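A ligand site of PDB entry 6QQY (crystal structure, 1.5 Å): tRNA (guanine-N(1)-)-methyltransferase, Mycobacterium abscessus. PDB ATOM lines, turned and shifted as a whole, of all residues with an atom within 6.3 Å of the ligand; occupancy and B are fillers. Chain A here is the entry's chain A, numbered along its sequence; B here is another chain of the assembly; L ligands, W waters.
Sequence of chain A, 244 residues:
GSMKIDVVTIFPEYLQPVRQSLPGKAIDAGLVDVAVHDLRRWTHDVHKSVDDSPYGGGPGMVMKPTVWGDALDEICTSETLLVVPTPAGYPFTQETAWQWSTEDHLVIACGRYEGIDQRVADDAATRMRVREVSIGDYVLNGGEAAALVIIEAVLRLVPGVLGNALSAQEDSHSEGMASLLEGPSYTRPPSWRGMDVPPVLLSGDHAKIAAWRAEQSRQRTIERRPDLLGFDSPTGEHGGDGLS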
ATOM      1  N   VAL A  84      -9.618  11.894  -1.432  1.00  0.00           N
ATOM      2  CA  VAL A  84      -8.231  11.947  -0.980  1.00  0.00           C
ATOM      3  C   VAL A  84      -7.299  11.420  -2.065  1.00  0.00           C
ATOM      4  O   VAL A  84      -7.128  10.200  -2.214  1.00  0.00           O
ATOM      5  CB  VAL A  84      -7.998  11.140   0.309  1.00  0.00           C
ATOM      6  CG1 VAL A  84      -6.593  11.385   0.844  1.00  0.00           C
ATOM      7  CG2 VAL A  84      -9.043  11.507   1.384  1.00  0.00           C
ATOM      8  N   PRO A  85      -6.681  12.319  -2.833  1.00  0.00           N
ATOM      9  CA  PRO A  85      -5.675  11.845  -3.786  1.00  0.00           C
ATOM     10  C   PRO A  85      -4.512  11.129  -3.099  1.00  0.00           C
ATOM     11  O   PRO A  85      -4.044  11.563  -2.025  1.00  0.00           O
ATOM     12  CB  PRO A  85      -5.204  13.140  -4.469  1.00  0.00           C
ATOM     13  CG  PRO A  85      -6.380  14.077  -4.354  1.00  0.00           C
ATOM     14  CD  PRO A  85      -7.005  13.749  -3.000  1.00  0.00           C
ATOM     15  N   THR A  86      -4.036  10.051  -3.718  1.00  0.00           N
ATOM     16  CA  THR A  86      -2.893   9.300  -3.223  1.00  0.00           C
ATOM     17  C   THR A  86      -2.417   8.387  -4.329  1.00  0.00           C
ATOM     18  O   THR A  86      -3.239   7.873  -5.080  1.00  0.00           O
ATOM     19  CB  THR A  86      -3.233   8.487  -1.938  1.00  0.00           C
ATOM     20  OG1 THR A  86      -2.257   7.448  -1.746  1.00  0.00           O
ATOM     21  CG2 THR A  86      -4.639   7.883  -2.008  1.00  0.00           C
ATOM     22  N   PRO A  87      -1.103   8.197  -4.431  1.00  0.00           N
ATOM     23  CA  PRO A  87      -0.593   7.275  -5.451  1.00  0.00           C
ATOM     24  C   PRO A  87      -1.054   5.835  -5.181  1.00  0.00           C
ATOM     25  O   PRO A  87      -1.005   5.024  -6.106  1.00  0.00           O
ATOM     26  CB  PRO A  87       0.936   7.417  -5.358  1.00  0.00           C
ATOM     27  CG  PRO A  87       1.197   8.053  -4.057  1.00  0.00           C
ATOM     28  CD  PRO A  87      -0.028   8.826  -3.647  1.00  0.00           C
ATOM     29  N   ALA A  88      -1.530   5.553  -3.964  1.00  0.00           N
ATOM     30  CA  ALA A  88      -2.034   4.232  -3.606  1.00  0.00           C
ATOM     31  C   ALA A  88      -3.560   4.109  -3.725  1.00  0.00           C
ATOM     32  O   ALA A  88      -4.160   3.159  -3.216  1.00  0.00           O
ATOM     33  CB  ALA A  88      -1.607   3.881  -2.173  1.00  0.00           C
ATOM     34  N   CYS A 110      -5.838  17.510   0.055  1.00  0.00           N
ATOM     35  CA  CYS A 110      -4.559  17.424  -0.645  1.00  0.00           C
ATOM     36  C   CYS A 110      -3.404  17.219   0.290  1.00  0.00           C
ATOM     37  O   CYS A 110      -3.082  18.100   1.092  1.00  0.00           O
ATOM     38  CB  CYS A 110      -4.290  18.698  -1.468  1.00  0.00           C
ATOM     39  SG  CYS A 110      -5.504  19.033  -2.740  1.00  0.00           S
ATOM     40  N   GLY A 111      -2.750  16.071   0.165  1.00  0.00           N
ATOM     41  CA  GLY A 111      -1.565  15.821   0.961  1.00  0.00           C
ATOM     42  C   GLY A 111      -0.292  16.310   0.314  1.00  0.00           C
ATOM     43  O   GLY A 111      -0.257  16.661  -0.860  1.00  0.00           O
ATOM     44  N   ARG A 112       0.746  16.325   1.126  1.00  0.00           N
ATOM     45  CA  ARG A 112       2.113  16.594   0.700  1.00  0.00           C
ATOM     46  C   ARG A 112       2.993  15.621   1.465  1.00  0.00           C
ATOM     47  O   ARG A 112       2.476  14.703   2.128  1.00  0.00           O
ATOM     48  CB  ARG A 112       2.488  18.058   0.948  1.00  0.00           C
ATOM     49  CG  ARG A 112       1.977  19.005  -0.160  1.00  0.00           C
ATOM     50  CD  ARG A 112       2.979  19.081  -1.318  1.00  0.00           C
ATOM     51  NE  ARG A 112       2.343  19.486  -2.567  1.00  0.00           N
ATOM     52  CZ  ARG A 112       2.996  19.846  -3.670  1.00  0.00           C
ATOM     53  NH1 ARG A 112       4.319  19.873  -3.673  1.00  0.00           N
ATOM     54  NH2 ARG A 112       2.312  20.195  -4.762  1.00  0.00           N
ATOM     55  N   TYR A 113       4.304  15.806   1.388  1.00  0.00           N
ATOM     56  CA  TYR A 113       5.240  14.912   2.074  1.00  0.00           C
ATOM     57  C   TYR A 113       4.986  13.482   1.594  1.00  0.00           C
ATOM     58  O   TYR A 113       4.822  13.272   0.383  1.00  0.00           O
ATOM     59  CB  TYR A 113       5.110  15.056   3.608  1.00  0.00           C
ATOM     60  CG  TYR A 113       5.256  16.491   4.096  1.00  0.00           C
ATOM     61  CD1 TYR A 113       6.499  17.012   4.432  1.00  0.00           C
ATOM     62  CD2 TYR A 113       4.154  17.328   4.198  1.00  0.00           C
ATOM     63  CE1 TYR A 113       6.642  18.321   4.857  1.00  0.00           C
ATOM     64  CE2 TYR A 113       4.287  18.644   4.615  1.00  0.00           C
ATOM     65  CZ  TYR A 113       5.536  19.130   4.955  1.00  0.00           C
ATOM     66  OH  TYR A 113       5.660  20.436   5.375  1.00  0.00           O
ATOM     67  N   GLU A 114       4.916  12.506   2.488  1.00  0.00           N
ATOM     68  CA  GLU A 114       4.640  11.123   2.068  1.00  0.00           C
ATOM     69  C   GLU A 114       3.185  10.695   2.240  1.00  0.00           C
ATOM     70  O   GLU A 114       2.859   9.502   2.144  1.00  0.00           O
ATOM     71  CB  GLU A 114       5.536  10.145   2.858  1.00  0.00           C
ATOM     72  CG  GLU A 114       7.024  10.357   2.668  1.00  0.00           C
ATOM     73  CD  GLU A 114       7.481  10.111   1.247  1.00  0.00           C
ATOM     74  OE1 GLU A 114       7.847  11.086   0.561  1.00  0.00           O
ATOM     75  OE2 GLU A 114       7.470   8.939   0.818  1.00  0.00           O
ATOM     76  N   GLY A 115       2.300  11.660   2.473  1.00  0.00           N
ATOM     77  CA  GLY A 115       0.882  11.382   2.594  1.00  0.00           C
ATOM     78  C   GLY A 115       0.343  11.724   3.976  1.00  0.00           C
ATOM     79  O   GLY A 115       1.048  12.320   4.802  1.00  0.00           O
ATOM     80  N   ILE A 116      -0.891  11.305   4.225  1.00  0.00           N
ATOM     81  CA  ILE A 116      -1.629  11.701   5.435  1.00  0.00           C
ATOM     82  C   ILE A 116      -1.778  10.483   6.328  1.00  0.00           C
ATOM     83  O   ILE A 116      -2.050   9.393   5.827  1.00  0.00           O
ATOM     84  CB  ILE A 116      -3.025  12.256   5.062  1.00  0.00           C
ATOM     85  CG1 ILE A 116      -2.891  13.436   4.087  1.00  0.00           C
ATOM     86  CG2 ILE A 116      -3.806  12.645   6.327  1.00  0.00           C
ATOM     87  CD1 ILE A 116      -4.203  13.931   3.541  1.00  0.00           C
ATOM     88  N   VAL A 133      -8.185   8.010  -4.120  1.00  0.00           N
ATOM     89  CA  VAL A 133      -8.060   7.767  -5.552  1.00  0.00           C
ATOM     90  C   VAL A 133      -6.737   8.257  -6.101  1.00  0.00           C
ATOM     91  O   VAL A 133      -6.119   9.168  -5.554  1.00  0.00           O
ATOM     92  CB  VAL A 133      -9.198   8.457  -6.369  1.00  0.00           C
ATOM     93  CG1 VAL A 133     -10.563   7.922  -5.960  1.00  0.00           C
ATOM     94  CG2 VAL A 133      -9.147   9.978  -6.210  1.00  0.00           C
ATOM     95  N   SER A 134      -6.329   7.657  -7.212  1.00  0.00           N
ATOM     96  CA  SER A 134      -5.126   8.047  -7.968  1.00  0.00           C
ATOM     97  C   SER A 134      -5.504   8.416  -9.395  1.00  0.00           C
ATOM     98  O   SER A 134      -6.252   7.677 -10.061  1.00  0.00           O
ATOM     99  CB  SER A 134      -4.125   6.899  -8.013  1.00  0.00           C
ATOM    100  OG  SER A 134      -3.079   7.206  -8.924  1.00  0.00           O
ATOM    101  N   ILE A 135      -4.915   9.514  -9.892  1.00  0.00           N
ATOM    102  CA  ILE A 135      -5.209   9.932 -11.273  1.00  0.00           C
ATOM    103  C   ILE A 135      -4.310   9.287 -12.346  1.00  0.00           C
ATOM    104  O   ILE A 135      -4.512   9.525 -13.536  1.00  0.00           O
ATOM    105  CB  ILE A 135      -5.118  11.471 -11.430  1.00  0.00           C
ATOM    106  CG1 ILE A 135      -3.717  11.990 -11.097  1.00  0.00           C
ATOM    107  CG2 ILE A 135      -6.195  12.173 -10.576  1.00  0.00           C
ATOM    108  CD1 ILE A 135      -3.410  13.376 -11.729  1.00  0.00           C
ATOM    109  N   GLY A 136      -3.361   8.453 -11.939  1.00  0.00           N
ATOM    110  CA  GLY A 136      -2.521   7.779 -12.919  1.00  0.00           C
ATOM    111  C   GLY A 136      -1.299   7.109 -12.338  1.00  0.00           C
ATOM    112  O   GLY A 136      -1.004   7.262 -11.151  1.00  0.00           O
ATOM    113  N   ASP A 137      -0.586   6.363 -13.165  1.00  0.00           N
ATOM    114  CA  ASP A 137       0.511   5.538 -12.683  1.00  0.00           C
ATOM    115  C   ASP A 137       1.848   6.252 -12.765  1.00  0.00           C
ATOM    116  O   ASP A 137       2.746   5.849 -13.497  1.00  0.00           O
ATOM    117  CB  ASP A 137       0.534   4.226 -13.453  1.00  0.00           C
ATOM    118  CG  ASP A 137      -0.664   3.350 -13.124  1.00  0.00           C
ATOM    119  OD1 ASP A 137      -1.208   3.499 -12.005  1.00  0.00           O
ATOM    120  OD2 ASP A 137      -1.060   2.523 -13.970  1.00  0.00           O
ATOM    121  N   TYR A 138       1.955   7.331 -12.002  1.00  0.00           N
ATOM    122  CA  TYR A 138       3.165   8.136 -11.886  1.00  0.00           C
ATOM    123  C   TYR A 138       3.086   8.758 -10.506  1.00  0.00           C
ATOM    124  O   TYR A 138       2.015   8.737  -9.894  1.00  0.00           O
ATOM    125  CB  TYR A 138       3.245   9.236 -12.965  1.00  0.00           C
ATOM    126  CG  TYR A 138       1.882   9.813 -13.276  1.00  0.00           C
ATOM    127  CD1 TYR A 138       1.286  10.741 -12.426  1.00  0.00           C
ATOM    128  CD2 TYR A 138       1.164   9.365 -14.382  1.00  0.00           C
ATOM    129  CE1 TYR A 138       0.032  11.233 -12.684  1.00  0.00           C
ATOM    130  CE2 TYR A 138      -0.098   9.858 -14.655  1.00  0.00           C
ATOM    131  CZ  TYR A 138      -0.665  10.791 -13.799  1.00  0.00           C
ATOM    132  OH  TYR A 138      -1.932  11.280 -14.045  1.00  0.00           O
ATOM    133  N   VAL A 139       4.202   9.282 -10.035  1.00  0.00           N
ATOM    134  CA  VAL A 139       4.277   9.852  -8.688  1.00  0.00           C
ATOM    135  C   VAL A 139       4.408  11.362  -8.769  1.00  0.00           C
ATOM    136  O   VAL A 139       5.253  11.883  -9.486  1.00  0.00           O
ATOM    137  CB  VAL A 139       5.469   9.265  -7.918  1.00  0.00           C
ATOM    138  CG1 VAL A 139       5.472   9.774  -6.485  1.00  0.00           C
ATOM    139  CG2 VAL A 139       5.411   7.746  -7.961  1.00  0.00           C
ATOM    140  N   LEU A 140       3.546  12.055  -8.024  1.00  0.00           N
ATOM    141  CA  LEU A 140       3.605  13.515  -7.894  1.00  0.00           C
ATOM    142  C   LEU A 140       4.208  13.877  -6.540  1.00  0.00           C
ATOM    143  O   LEU A 140       4.499  12.993  -5.739  1.00  0.00           O
ATOM    144  CB  LEU A 140       2.207  14.109  -8.021  1.00  0.00           C
ATOM    145  CG  LEU A 140       1.497  13.764  -9.336  1.00  0.00           C
ATOM    146  CD1 LEU A 140       0.021  14.117  -9.252  1.00  0.00           C
ATOM    147  CD2 LEU A 140       2.168  14.489 -10.491  1.00  0.00           C
ATOM    148  N   ASN A 141       4.375  15.174  -6.294  1.00  0.00           N
ATOM    149  CA  ASN A 141       4.878  15.635  -4.990  1.00  0.00           C
ATOM    150  C   ASN A 141       3.762  15.825  -3.963  1.00  0.00           C
ATOM    151  O   ASN A 141       4.019  15.948  -2.767  1.00  0.00           O
ATOM    152  CB  ASN A 141       5.634  16.951  -5.129  1.00  0.00           C
ATOM    153  CG  ASN A 141       6.976  16.782  -5.806  1.00  0.00           C
ATOM    154  OD1 ASN A 141       7.706  15.834  -5.528  1.00  0.00           O
ATOM    155  ND2 ASN A 141       7.314  17.714  -6.694  1.00  0.00           N
ATOM    156  N   GLY A 142       2.509  15.852  -4.427  1.00  0.00           N
ATOM    157  CA  GLY A 142       1.387  16.091  -3.547  1.00  0.00           C
ATOM    158  C   GLY A 142       0.087  16.022  -4.311  1.00  0.00           C
ATOM    159  O   GLY A 142       0.087  15.790  -5.535  1.00  0.00           O
ATOM    160  N   GLY A 143      -1.019  16.239  -3.607  1.00  0.00           N
ATOM    161  CA  GLY A 143      -2.339  16.054  -4.196  1.00  0.00           C
ATOM    162  C   GLY A 143      -2.914  17.199  -5.018  1.00  0.00           C
ATOM    163  O   GLY A 143      -3.968  17.022  -5.630  1.00  0.00           O
ATOM    164  N   GLU A 144      -2.252  18.358  -5.031  1.00  0.00           N
ATOM    165  CA  GLU A 144      -2.828  19.541  -5.659  1.00  0.00           C
ATOM    166  C   GLU A 144      -3.046  19.378  -7.166  1.00  0.00           C
ATOM    167  O   GLU A 144      -4.109  19.726  -7.674  1.00  0.00           O
ATOM    168  CB  GLU A 144      -1.937  20.766  -5.410  1.00  0.00           C
ATOM    169  CG  GLU A 144      -1.988  21.255  -3.956  1.00  0.00           C
ATOM    170  CD  GLU A 144      -1.143  20.429  -2.986  1.00  0.00           C
ATOM    171  OE1 GLU A 144      -0.336  19.584  -3.422  1.00  0.00           O
ATOM    172  OE2 GLU A 144      -1.279  20.669  -1.768  1.00  0.00           O
ATOM    173  N   ALA A 146      -3.420  16.623  -8.726  1.00  0.00           N
ATOM    174  CA  ALA A 146      -4.515  15.645  -8.835  1.00  0.00           C
ATOM    175  C   ALA A 146      -5.883  16.298  -8.611  1.00  0.00           C
ATOM    176  O   ALA A 146      -6.847  15.983  -9.319  1.00  0.00           O
ATOM    177  CB  ALA A 146      -4.301  14.495  -7.856  1.00  0.00           C
ATOM    178  N   ILE A 150      -9.045  16.279 -11.124  1.00  0.00           N
ATOM    179  CA  ILE A 150     -10.342  15.783 -10.680  1.00  0.00           C
ATOM    180  C   ILE A 150     -11.424  16.859 -10.808  1.00  0.00           C
ATOM    181  O   ILE A 150     -12.528  16.588 -11.313  1.00  0.00           O
ATOM    182  CB  ILE A 150     -10.256  15.270  -9.226  1.00  0.00           C
ATOM    183  CG1 ILE A 150      -9.423  13.969  -9.190  1.00  0.00           C
ATOM    184  CG2 ILE A 150     -11.648  15.034  -8.676  1.00  0.00           C
ATOM    185  CD1 ILE A 150      -8.938  13.575  -7.795  1.00  0.00           C
ATOM    186  N   ARG B 156      10.597  16.205 -10.523  1.00  0.00           N
ATOM    187  CA  ARG B 156      11.030  15.631  -9.246  1.00  0.00           C
ATOM    188  C   ARG B 156      12.062  14.512  -9.448  1.00  0.00           C
ATOM    189  O   ARG B 156      12.685  14.055  -8.494  1.00  0.00           O
ATOM    190  CB  ARG B 156       9.817  15.133  -8.450  1.00  0.00           C
ATOM    191  CG  ARG B 156       9.001  14.046  -9.122  1.00  0.00           C
ATOM    192  CD  ARG B 156       7.699  13.806  -8.335  1.00  0.00           C
ATOM    193  NE  ARG B 156       7.933  13.348  -6.974  1.00  0.00           N
ATOM    194  CZ  ARG B 156       8.308  12.116  -6.651  1.00  0.00           C
ATOM    195  NH1 ARG B 156       8.541  11.202  -7.611  1.00  0.00           N
ATOM    196  NH2 ARG B 156       8.478  11.777  -5.380  1.00  0.00           N
ATOM    197  N   GLU B 182       1.709   1.874  -2.222  1.00  0.00           N
ATOM    198  CA  GLU B 182       2.187   2.189  -0.879  1.00  0.00           C
ATOM    199  C   GLU B 182       1.146   1.797   0.166  1.00  0.00           C
ATOM    200  O   GLU B 182      -0.052   1.984  -0.043  1.00  0.00           O
ATOM    201  CB  GLU B 182       2.516   3.678  -0.761  1.00  0.00           C
ATOM    202  CG  GLU B 182       3.605   4.171  -1.694  1.00  0.00           C
ATOM    203  CD  GLU B 182       3.119   4.479  -3.102  1.00  0.00           C
ATOM    204  OE1 GLU B 182       1.949   4.161  -3.423  1.00  0.00           O
ATOM    205  OE2 GLU B 182       3.909   5.038  -3.883  1.00  0.00           O
HETATM  206  C1  LIG L   1       1.190  12.563  -3.124  1.00  0.00           C
HETATM  207  C2  LIG L   1       4.002  11.030  -2.305  1.00  0.00           C
HETATM  208  C3  LIG L   1       3.483   9.004  -1.323  1.00  0.00           C
HETATM  209  C4  LIG L   1       5.532   9.204  -2.586  1.00  0.00           C
HETATM  210  C5  LIG L   1       0.416  13.460  -1.193  1.00  0.00           C
HETATM  211  C6  LIG L   1       1.152  12.033  -4.435  1.00  0.00           C
HETATM  212  C7  LIG L   1      -1.192  10.850  -7.223  1.00  0.00           C
HETATM  213  N1  LIG L   1      -1.343   9.629  -9.403  1.00  0.00           N
HETATM  214  C8  LIG L   1      -0.635  10.222  -8.322  1.00  0.00           C
HETATM  215  N2  LIG L   1       0.710  10.233  -8.184  1.00  0.00           N
HETATM  216  N3  LIG L   1       1.012  10.877  -7.020  1.00  0.00           N
HETATM  217  C9  LIG L   1      -0.120  11.283  -6.447  1.00  0.00           C
HETATM  218  C10 LIG L   1      -0.101  11.948  -5.076  1.00  0.00           C
HETATM  219  C11 LIG L   1      -1.302  12.327  -4.455  1.00  0.00           C
HETATM  220  C12 LIG L   1      -1.249  12.846  -3.157  1.00  0.00           C
HETATM  221  C13 LIG L   1       0.015  12.969  -2.502  1.00  0.00           C
HETATM  222  N4  LIG L   1       2.251  12.797  -2.276  1.00  0.00           N
HETATM  223  C14 LIG L   1       3.644  12.492  -2.576  1.00  0.00           C
HETATM  224  N5  LIG L   1       3.201  10.271  -1.584  1.00  0.00           N
HETATM  225  C15 LIG L   1       4.649   8.430  -1.818  1.00  0.00           C
HETATM  226  C16 LIG L   1       5.191  10.545  -2.834  1.00  0.00           C
HETATM  227  C17 LIG L   1       1.811  13.327  -1.109  1.00  0.00           C
HETATM  228  C18 LIG L   1      -2.685  11.024  -7.059  1.00  0.00           C
HETATM  229  N6  LIG L   1      -3.824  11.125  -7.006  1.00  0.00           N
HETATM  230  O   HOH W   1      -2.001  11.546   0.298  1.00  0.00           O
HETATM  231  O   HOH W   2       0.396  10.169  -0.516  1.00  0.00           O
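N6 of the ligand sits close to O of Val 133. Merely in contact with the ligand: Pro 85, Pro 87, Gly 111, Arg 112, Tyr 113, Glu 114, Gly 115, Val 139, Asn 141, Gly 142, Gly 143 and Ala 146. Hydrophobic or aromatic side chains that line the ligand: Pro 85, Pro 87, Ile 135, Tyr 138, Val 139, Leu 140 and Ala 146. 19 residues have an atom within 4 Å of the ligand: Pro 85, Thr 86, Pro 87, Gly 111, Arg 112, Tyr 113, Glu 114, Gly 115, Val 133, Ser 134, Ile 135, Gly 136, Tyr 138, Val 139, Leu 140, Asn 141, Gly 142, Gly 143 and Ala 146. The nearest printed residue that does not touch the ligand is Glu 182 of chain B (4.04 Å).
O of Gly 111 sits at hydrogen-bond distance from N of Gly 143, at 2.9 Å. The side-chain hydroxyl (OG) of Ser 134 lies within hydrogen-bond range of the backbone carbonyl oxygen (O) of Gly 136 (3.0 Å). OH of Tyr 138 sits at hydrogen-bond distance from O of Ile 135, at 3.2 Å. The guanidinium group (NE) of Arg 156 of chain B sits at hydrogen-bond distance from the side-chain amide oxygen (OD1) of Asn 141, at 2.9 Å. The backbone carbonyl oxygen of Val 84 lies within hydrogen-bond range of the backbone NH of Val 133 (3.1 Å). The backbone carbonyl oxygen of Val 133 is in hydrogen-bond range of the backbone NH of Thr 86 (2.9 Å). The backbone NH (N) of Ala 88 lies close to the side-chain hydroxyl (OG1) of Thr 86 (3.0 Å). The guanidinium group (NE) of Arg 112 is in salt-bridge range of the side-chain carboxylate (OE1) of Glu 144, 2.8 Å away.
O of Gly 136 is in hydrogen-bond range of N1 of the ligand, 3.0 Å away. N of Ile 135 sits at hydrogen-bond distance from N6 of the ligand, 3.5 Å away. OG of Ser 134 is in hydrogen-bond range of N1 of the ligand, 3.0 Å away. The backbone NH (N) of Thr 86 is in hydrogen-bond range of a nitrogen (N6) of the ligand, 3.5 Å away. N of Leu 140 is in hydrogen-bond range of N3 of the ligand. O of Tyr 138 sits at hydrogen-bond distance from N2 of the ligand (2.6 Å).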
